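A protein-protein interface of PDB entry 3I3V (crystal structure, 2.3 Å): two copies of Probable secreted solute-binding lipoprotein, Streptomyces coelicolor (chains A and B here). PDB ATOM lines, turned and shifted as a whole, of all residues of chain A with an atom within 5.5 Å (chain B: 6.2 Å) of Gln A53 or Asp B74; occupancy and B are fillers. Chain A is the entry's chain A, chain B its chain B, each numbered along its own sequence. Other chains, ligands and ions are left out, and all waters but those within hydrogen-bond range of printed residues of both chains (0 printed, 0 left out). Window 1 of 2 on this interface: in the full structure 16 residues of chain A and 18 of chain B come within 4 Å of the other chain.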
ATOM      1  N   ASP A  49      17.799  -2.735  -8.338  1.00  0.00           N
ATOM      2  CA  ASP A  49      17.757  -1.298  -8.092  1.00  0.00           C
ATOM      3  C   ASP A  49      16.896  -0.535  -9.080  1.00  0.00           C
ATOM      4  O   ASP A  49      16.583   0.634  -8.869  1.00  0.00           O
ATOM      5  CB  ASP A  49      19.172  -0.710  -8.092  1.00  0.00           C
ATOM      6  CG  ASP A  49      19.864  -0.853  -6.738  1.00  0.00           C
ATOM      7  OD1 ASP A  49      20.950  -0.259  -6.554  1.00  0.00           O
ATOM      8  OD2 ASP A  49      19.322  -1.561  -5.856  1.00  0.00           O
ATOM      9  N   ASP A  50      16.498  -1.194 -10.154  1.00  0.00           N
ATOM     10  CA  ASP A  50      15.684  -0.530 -11.148  1.00  0.00           C
ATOM     11  C   ASP A  50      14.209  -0.889 -11.040  1.00  0.00           C
ATOM     12  O   ASP A  50      13.442  -0.619 -11.963  1.00  0.00           O
ATOM     13  CB  ASP A  50      16.197  -0.880 -12.545  1.00  0.00           C
ATOM     14  CG  ASP A  50      16.026  -2.347 -12.873  1.00  0.00           C
ATOM     15  OD1 ASP A  50      16.347  -3.192 -12.004  1.00  0.00           O
ATOM     16  OD2 ASP A  50      15.574  -2.655 -13.998  1.00  0.00           O
ATOM     17  N   LEU A  51      13.799  -1.486  -9.924  1.00  0.00           N
ATOM     18  CA  LEU A  51      12.398  -1.874  -9.776  1.00  0.00           C
ATOM     19  C   LEU A  51      11.481  -0.663  -9.792  1.00  0.00           C
ATOM     20  O   LEU A  51      10.483  -0.648 -10.519  1.00  0.00           O
ATOM     21  CB  LEU A  51      12.167  -2.689  -8.485  1.00  0.00           C
ATOM     22  CG  LEU A  51      10.707  -3.133  -8.221  1.00  0.00           C
ATOM     23  CD1 LEU A  51      10.674  -4.392  -7.331  1.00  0.00           C
ATOM     24  CD2 LEU A  51       9.917  -1.981  -7.592  1.00  0.00           C
ATOM     25  N   ALA A  52      11.822   0.348  -8.997  1.00  0.00           N
ATOM     26  CA  ALA A  52      11.016   1.561  -8.923  1.00  0.00           C
ATOM     27  C   ALA A  52      10.746   2.127 -10.306  1.00  0.00           C
ATOM     28  O   ALA A  52       9.609   2.508 -10.606  1.00  0.00           O
ATOM     29  CB  ALA A  52      11.705   2.603  -8.047  1.00  0.00           C
ATOM     30  N   GLN A  53      11.779   2.171 -11.151  1.00  0.00           N
ATOM     31  CA  GLN A  53      11.643   2.679 -12.518  1.00  0.00           C
ATOM     32  C   GLN A  53      10.801   1.752 -13.396  1.00  0.00           C
ATOM     33  O   GLN A  53       9.974   2.204 -14.194  1.00  0.00           O
ATOM     34  CB  GLN A  53      13.020   2.874 -13.178  1.00  0.00           C
ATOM     35  CG  GLN A  53      13.888   3.938 -12.506  1.00  0.00           C
ATOM     36  CD  GLN A  53      14.954   3.345 -11.593  1.00  0.00           C
ATOM     37  OE1 GLN A  53      16.117   3.184 -11.995  1.00  0.00           O
ATOM     38  NE2 GLN A  53      14.561   3.005 -10.364  1.00  0.00           N
ATOM     39  N   VAL A  54      11.016   0.449 -13.271  1.00  0.00           N
ATOM     40  CA  VAL A  54      10.236  -0.484 -14.076  1.00  0.00           C
ATOM     41  C   VAL A  54       8.781  -0.440 -13.629  1.00  0.00           C
ATOM     42  O   VAL A  54       7.874  -0.578 -14.443  1.00  0.00           O
ATOM     43  CB  VAL A  54      10.774  -1.927 -13.957  1.00  0.00           C
ATOM     44  CG1 VAL A  54       9.870  -2.899 -14.713  1.00  0.00           C
ATOM     45  CG2 VAL A  54      12.169  -1.990 -14.523  1.00  0.00           C
ATOM     46  N   TYR A  55       8.563  -0.228 -12.335  1.00  0.00           N
ATOM     47  CA  TYR A  55       7.201  -0.166 -11.815  1.00  0.00           C
ATOM     48  C   TYR A  55       6.459   1.076 -12.315  1.00  0.00           C
ATOM     49  O   TYR A  55       5.302   0.983 -12.751  1.00  0.00           O
ATOM     50  CB  TYR A  55       7.197  -0.170 -10.285  1.00  0.00           C
ATOM     51  CG  TYR A  55       5.816   0.075  -9.689  1.00  0.00           C
ATOM     52  CD1 TYR A  55       4.829  -0.919  -9.706  1.00  0.00           C
ATOM     53  CD2 TYR A  55       5.487   1.321  -9.145  1.00  0.00           C
ATOM     54  CE1 TYR A  55       3.550  -0.674  -9.195  1.00  0.00           C
ATOM     55  CE2 TYR A  55       4.216   1.573  -8.639  1.00  0.00           C
ATOM     56  CZ  TYR A  55       3.257   0.578  -8.665  1.00  0.00           C
ATOM     57  OH  TYR A  55       2.008   0.856  -8.162  1.00  0.00           O
ATOM     58  N   GLU A  56       7.110   2.235 -12.246  1.00  0.00           N
ATOM     59  CA  GLU A  56       6.464   3.469 -12.689  1.00  0.00           C
ATOM     60  C   GLU A  56       6.087   3.364 -14.164  1.00  0.00           C
ATOM     61  O   GLU A  56       5.067   3.911 -14.594  1.00  0.00           O
ATOM     62  CB  GLU A  56       7.368   4.684 -12.423  1.00  0.00           C
ATOM     63  CG  GLU A  56       7.449   5.042 -10.935  1.00  0.00           C
ATOM     64  CD  GLU A  56       8.691   5.847 -10.564  1.00  0.00           C
ATOM     65  OE1 GLU A  56       9.541   6.112 -11.443  1.00  0.00           O
ATOM     66  OE2 GLU A  56       8.823   6.217  -9.374  1.00  0.00           O
ATOM     67  N   THR A  57       6.896   2.641 -14.931  1.00  0.00           N
ATOM     68  CA  THR A  57       6.609   2.455 -16.345  1.00  0.00           C
ATOM     69  C   THR A  57       5.406   1.525 -16.550  1.00  0.00           C
ATOM     70  O   THR A  57       4.601   1.741 -17.449  1.00  0.00           O
ATOM     71  CB  THR A  57       7.821   1.878 -17.095  1.00  0.00           C
ATOM     72  OG1 THR A  57       8.863   2.862 -17.147  1.00  0.00           O
ATOM     73  CG2 THR A  57       7.433   1.492 -18.504  1.00  0.00           C
ATOM     74  N   SER A  58       5.279   0.487 -15.725  1.00  0.00           N
ATOM     75  CA  SER A  58       4.149  -0.416 -15.874  1.00  0.00           C
ATOM     76  C   SER A  58       2.882   0.320 -15.454  1.00  0.00           C
ATOM     77  O   SER A  58       1.780  -0.021 -15.870  1.00  0.00           O
ATOM     78  CB  SER A  58       4.340  -1.677 -15.024  1.00  0.00           C
ATOM     79  OG  SER A  58       4.203  -1.406 -13.639  1.00  0.00           O
ATOM     80  N   TYR A  73      13.278   4.648  -0.011  1.00  0.00           N
ATOM     81  CA  TYR A  73      14.410   5.498  -0.345  1.00  0.00           C
ATOM     82  C   TYR A  73      13.851   6.616  -1.223  1.00  0.00           C
ATOM     83  O   TYR A  73      12.659   6.606  -1.531  1.00  0.00           O
ATOM     84  CB  TYR A  73      15.516   4.706  -1.059  1.00  0.00           C
ATOM     85  CG  TYR A  73      15.205   4.265  -2.469  1.00  0.00           C
ATOM     86  CD1 TYR A  73      14.250   3.280  -2.724  1.00  0.00           C
ATOM     87  CD2 TYR A  73      15.898   4.800  -3.550  1.00  0.00           C
ATOM     88  CE1 TYR A  73      14.001   2.832  -4.018  1.00  0.00           C
ATOM     89  CE2 TYR A  73      15.651   4.362  -4.857  1.00  0.00           C
ATOM     90  CZ  TYR A  73      14.705   3.379  -5.080  1.00  0.00           C
ATOM     91  OH  TYR A  73      14.467   2.941  -6.367  1.00  0.00           O
ATOM     92  N   LYS A  75      13.364   7.413  -4.320  1.00  0.00           N
ATOM     93  CA  LYS A  75      12.416   7.196  -5.406  1.00  0.00           C
ATOM     94  C   LYS A  75      11.026   6.743  -4.966  1.00  0.00           C
ATOM     95  O   LYS A  75      10.028   7.132  -5.581  1.00  0.00           O
ATOM     96  CB  LYS A  75      12.982   6.205  -6.419  1.00  0.00           C
ATOM     97  CG  LYS A  75      13.905   6.861  -7.421  1.00  0.00           C
ATOM     98  CD  LYS A  75      14.329   5.891  -8.507  1.00  0.00           C
ATOM     99  CE  LYS A  75      15.133   6.619  -9.578  1.00  0.00           C
ATOM    100  NZ  LYS A  75      16.190   7.483  -8.975  1.00  0.00           N
ATOM    101  N   LEU B  72      17.507  12.953 -22.577  1.00  0.00           N
ATOM    102  CA  LEU B  72      17.248  11.531 -22.747  1.00  0.00           C
ATOM    103  C   LEU B  72      18.075  10.740 -21.750  1.00  0.00           C
ATOM    104  O   LEU B  72      19.298  10.712 -21.823  1.00  0.00           O
ATOM    105  CB  LEU B  72      17.581  11.074 -24.178  1.00  0.00           C
ATOM    106  CG  LEU B  72      17.149   9.642 -24.549  1.00  0.00           C
ATOM    107  CD1 LEU B  72      15.638   9.532 -24.421  1.00  0.00           C
ATOM    108  CD2 LEU B  72      17.593   9.291 -25.982  1.00  0.00           C
ATOM    109  N   TYR B  73      17.393  10.116 -20.798  1.00  0.00           N
ATOM    110  CA  TYR B  73      18.063   9.321 -19.798  1.00  0.00           C
ATOM    111  C   TYR B  73      17.129   8.192 -19.388  1.00  0.00           C
ATOM    112  O   TYR B  73      16.028   8.054 -19.925  1.00  0.00           O
ATOM    113  CB  TYR B  73      18.446  10.173 -18.579  1.00  0.00           C
ATOM    114  CG  TYR B  73      17.284  10.603 -17.708  1.00  0.00           C
ATOM    115  CD1 TYR B  73      16.361  11.542 -18.155  1.00  0.00           C
ATOM    116  CD2 TYR B  73      17.105  10.060 -16.432  1.00  0.00           C
ATOM    117  CE1 TYR B  73      15.280  11.931 -17.352  1.00  0.00           C
ATOM    118  CE2 TYR B  73      16.029  10.444 -15.618  1.00  0.00           C
ATOM    119  CZ  TYR B  73      15.124  11.377 -16.088  1.00  0.00           C
ATOM    120  OH  TYR B  73      14.057  11.761 -15.312  1.00  0.00           O
ATOM    121  N   ASP B  74      17.581   7.393 -18.434  1.00  0.00           N
ATOM    122  CA  ASP B  74      16.840   6.250 -17.933  1.00  0.00           C
ATOM    123  C   ASP B  74      15.310   6.334 -17.999  1.00  0.00           C
ATOM    124  O   ASP B  74      14.674   5.598 -18.751  1.00  0.00           O
ATOM    125  CB  ASP B  74      17.262   5.970 -16.493  1.00  0.00           C
ATOM    126  CG  ASP B  74      16.751   4.639 -15.995  1.00  0.00           C
ATOM    127  OD1 ASP B  74      16.055   4.615 -14.955  1.00  0.00           O
ATOM    128  OD2 ASP B  74      17.049   3.620 -16.653  1.00  0.00           O
ATOM    129  N   LYS B  75      14.715   7.230 -17.219  1.00  0.00           N
ATOM    130  CA  LYS B  75      13.262   7.331 -17.195  1.00  0.00           C
ATOM    131  C   LYS B  75      12.586   7.725 -18.518  1.00  0.00           C
ATOM    132  O   LYS B  75      11.610   7.089 -18.912  1.00  0.00           O
ATOM    133  CB  LYS B  75      12.827   8.259 -16.048  1.00  0.00           C
ATOM    134  CG  LYS B  75      11.319   8.389 -15.878  1.00  0.00           C
ATOM    135  CD  LYS B  75      10.906   8.414 -14.407  1.00  0.00           C
ATOM    136  CE  LYS B  75      10.201   7.111 -14.048  1.00  0.00           C
ATOM    137  NZ  LYS B  75      11.020   5.919 -14.481  1.00  0.00           N
ATOM    138  N   THR B  76      13.094   8.734 -19.226  1.00  0.00           N
ATOM    139  CA  THR B  76      12.448   9.129 -20.478  1.00  0.00           C
ATOM    140  C   THR B  76      12.730   8.182 -21.645  1.00  0.00           C
ATOM    141  O   THR B  76      12.073   8.248 -22.681  1.00  0.00           O
ATOM    142  CB  THR B  76      12.825  10.580 -20.887  1.00  0.00           C
ATOM    143  OG1 THR B  76      14.237  10.674 -21.100  1.00  0.00           O
ATOM    144  CG2 THR B  76      12.409  11.560 -19.794  1.00  0.00           C
ATOM    145  N   LEU B  77      13.690   7.288 -21.465  1.00  0.00           N
ATOM    146  CA  LEU B  77      14.050   6.322 -22.497  1.00  0.00           C
ATOM    147  C   LEU B  77      12.908   5.321 -22.718  1.00  0.00           C
ATOM    148  O   LEU B  77      12.878   4.612 -23.722  1.00  0.00           O
ATOM    149  CB  LEU B  77      15.320   5.583 -22.059  1.00  0.00           C
ATOM    150  CG  LEU B  77      16.497   5.303 -23.004  1.00  0.00           C
ATOM    151  CD1 LEU B  77      16.470   6.189 -24.229  1.00  0.00           C
ATOM    152  CD2 LEU B  77      17.781   5.515 -22.224  1.00  0.00           C
ATOM    153  N   ALA B  78      11.958   5.294 -21.784  1.00  0.00           N
ATOM    154  CA  ALA B  78      10.822   4.372 -21.830  1.00  0.00           C
ATOM    155  C   ALA B  78       9.496   5.003 -22.237  1.00  0.00           C
ATOM    156  O   ALA B  78       8.530   4.299 -22.527  1.00  0.00           O
ATOM    157  CB  ALA B  78      10.659   3.702 -20.474  1.00  0.00           C
ATOM    158  N   VAL B 359      23.824   7.669 -21.078  1.00  0.00           N
ATOM    159  CA  VAL B 359      22.587   6.985 -21.461  1.00  0.00           C
ATOM    160  C   VAL B 359      22.606   5.461 -21.382  1.00  0.00           C
ATOM    161  O   VAL B 359      21.637   4.848 -20.944  1.00  0.00           O
ATOM    162  CB  VAL B 359      22.127   7.362 -22.897  1.00  0.00           C
ATOM    163  CG1 VAL B 359      21.086   8.449 -22.842  1.00  0.00           C
ATOM    164  CG2 VAL B 359      23.304   7.805 -23.727  1.00  0.00           C
ATOM    165  N   PRO B 362      23.703   1.393 -16.954  1.00  0.00           N
ATOM    166  CA  PRO B 362      22.536   1.195 -16.085  1.00  0.00           C
ATOM    167  C   PRO B 362      22.704   2.057 -14.843  1.00  0.00           C
ATOM    168  O   PRO B 362      23.801   2.164 -14.306  1.00  0.00           O
ATOM    169  CB  PRO B 362      22.595  -0.293 -15.757  1.00  0.00           C
ATOM    170  CG  PRO B 362      23.253  -0.874 -16.949  1.00  0.00           C
ATOM    171  CD  PRO B 362      24.365   0.109 -17.232  1.00  0.00           C
ATOM    172  N   PRO B 363      21.619   2.680 -14.370  1.00  0.00           N
ATOM    173  CA  PRO B 363      21.694   3.531 -13.181  1.00  0.00           C
ATOM    174  C   PRO B 363      22.403   2.908 -11.973  1.00  0.00           C
ATOM    175  O   PRO B 363      23.173   3.579 -11.283  1.00  0.00           O
ATOM    176  CB  PRO B 363      20.228   3.842 -12.900  1.00  0.00           C
ATOM    177  CG  PRO B 363      19.630   3.878 -14.280  1.00  0.00           C
ATOM    178  CD  PRO B 363      20.249   2.654 -14.914  1.00  0.00           C
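The side-chain amide oxygen (OE1) of Gln A53 sits close to the side-chain carboxylate (OD1) of Asp B74 (3.3 Å).
OE1 of Glu A56 lies within salt-bridge range of NZ of Lys B75 (3.4 Å).
OG1 of Thr A57 is in hydrogen-bond range of O of Gln A53 (3.2 Å).
O of Asp A49 is in hydrogen-bond range of NE2 of Gln A53 (3.5 Å).
Among the printed residues, merely in contact across the chains: Gln A53 with Lys B75 (3.8 Å) and Thr A57 with Ala B78 (3.9 Å).
Of the printed residues of chain B, Gln A53 touches Asp B74 and Lys B75.
Printed residues of chain B within 4 Å of Glu A56: Lys B75.
Of the printed residues of chain A, Asp B74 touches Gln A53.
Printed residues of chain A within 4 Å of Lys B75: Gln A53 (3.8 Å) and Glu A56 (2.9 Å).
The nearest residue of chain B that does not touch Gln A53 is Pro B363 (4.2 Å).
The nearest printed residue of chain B that does not touch Thr A57 is Lys B75 (4.6 Å).
Of the 10 printed residues of chain B, 3 touch a printed residue of chain A.
Printed residues of chain B that touch a printed residue of chain A: Asp B74, Lys B75 and Ala B78.
Hydrophobic or aromatic side chains of chain B that line the printed part of chain A: Ala B78.
Among the printed residues, Asp or Glu carboxylates within 4 Å of a Lys or Arg side-chain nitrogen of the other chain: Glu A56 with Lys B75 (3.4 Å).
Positions printed for both chains: 73 and 75.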
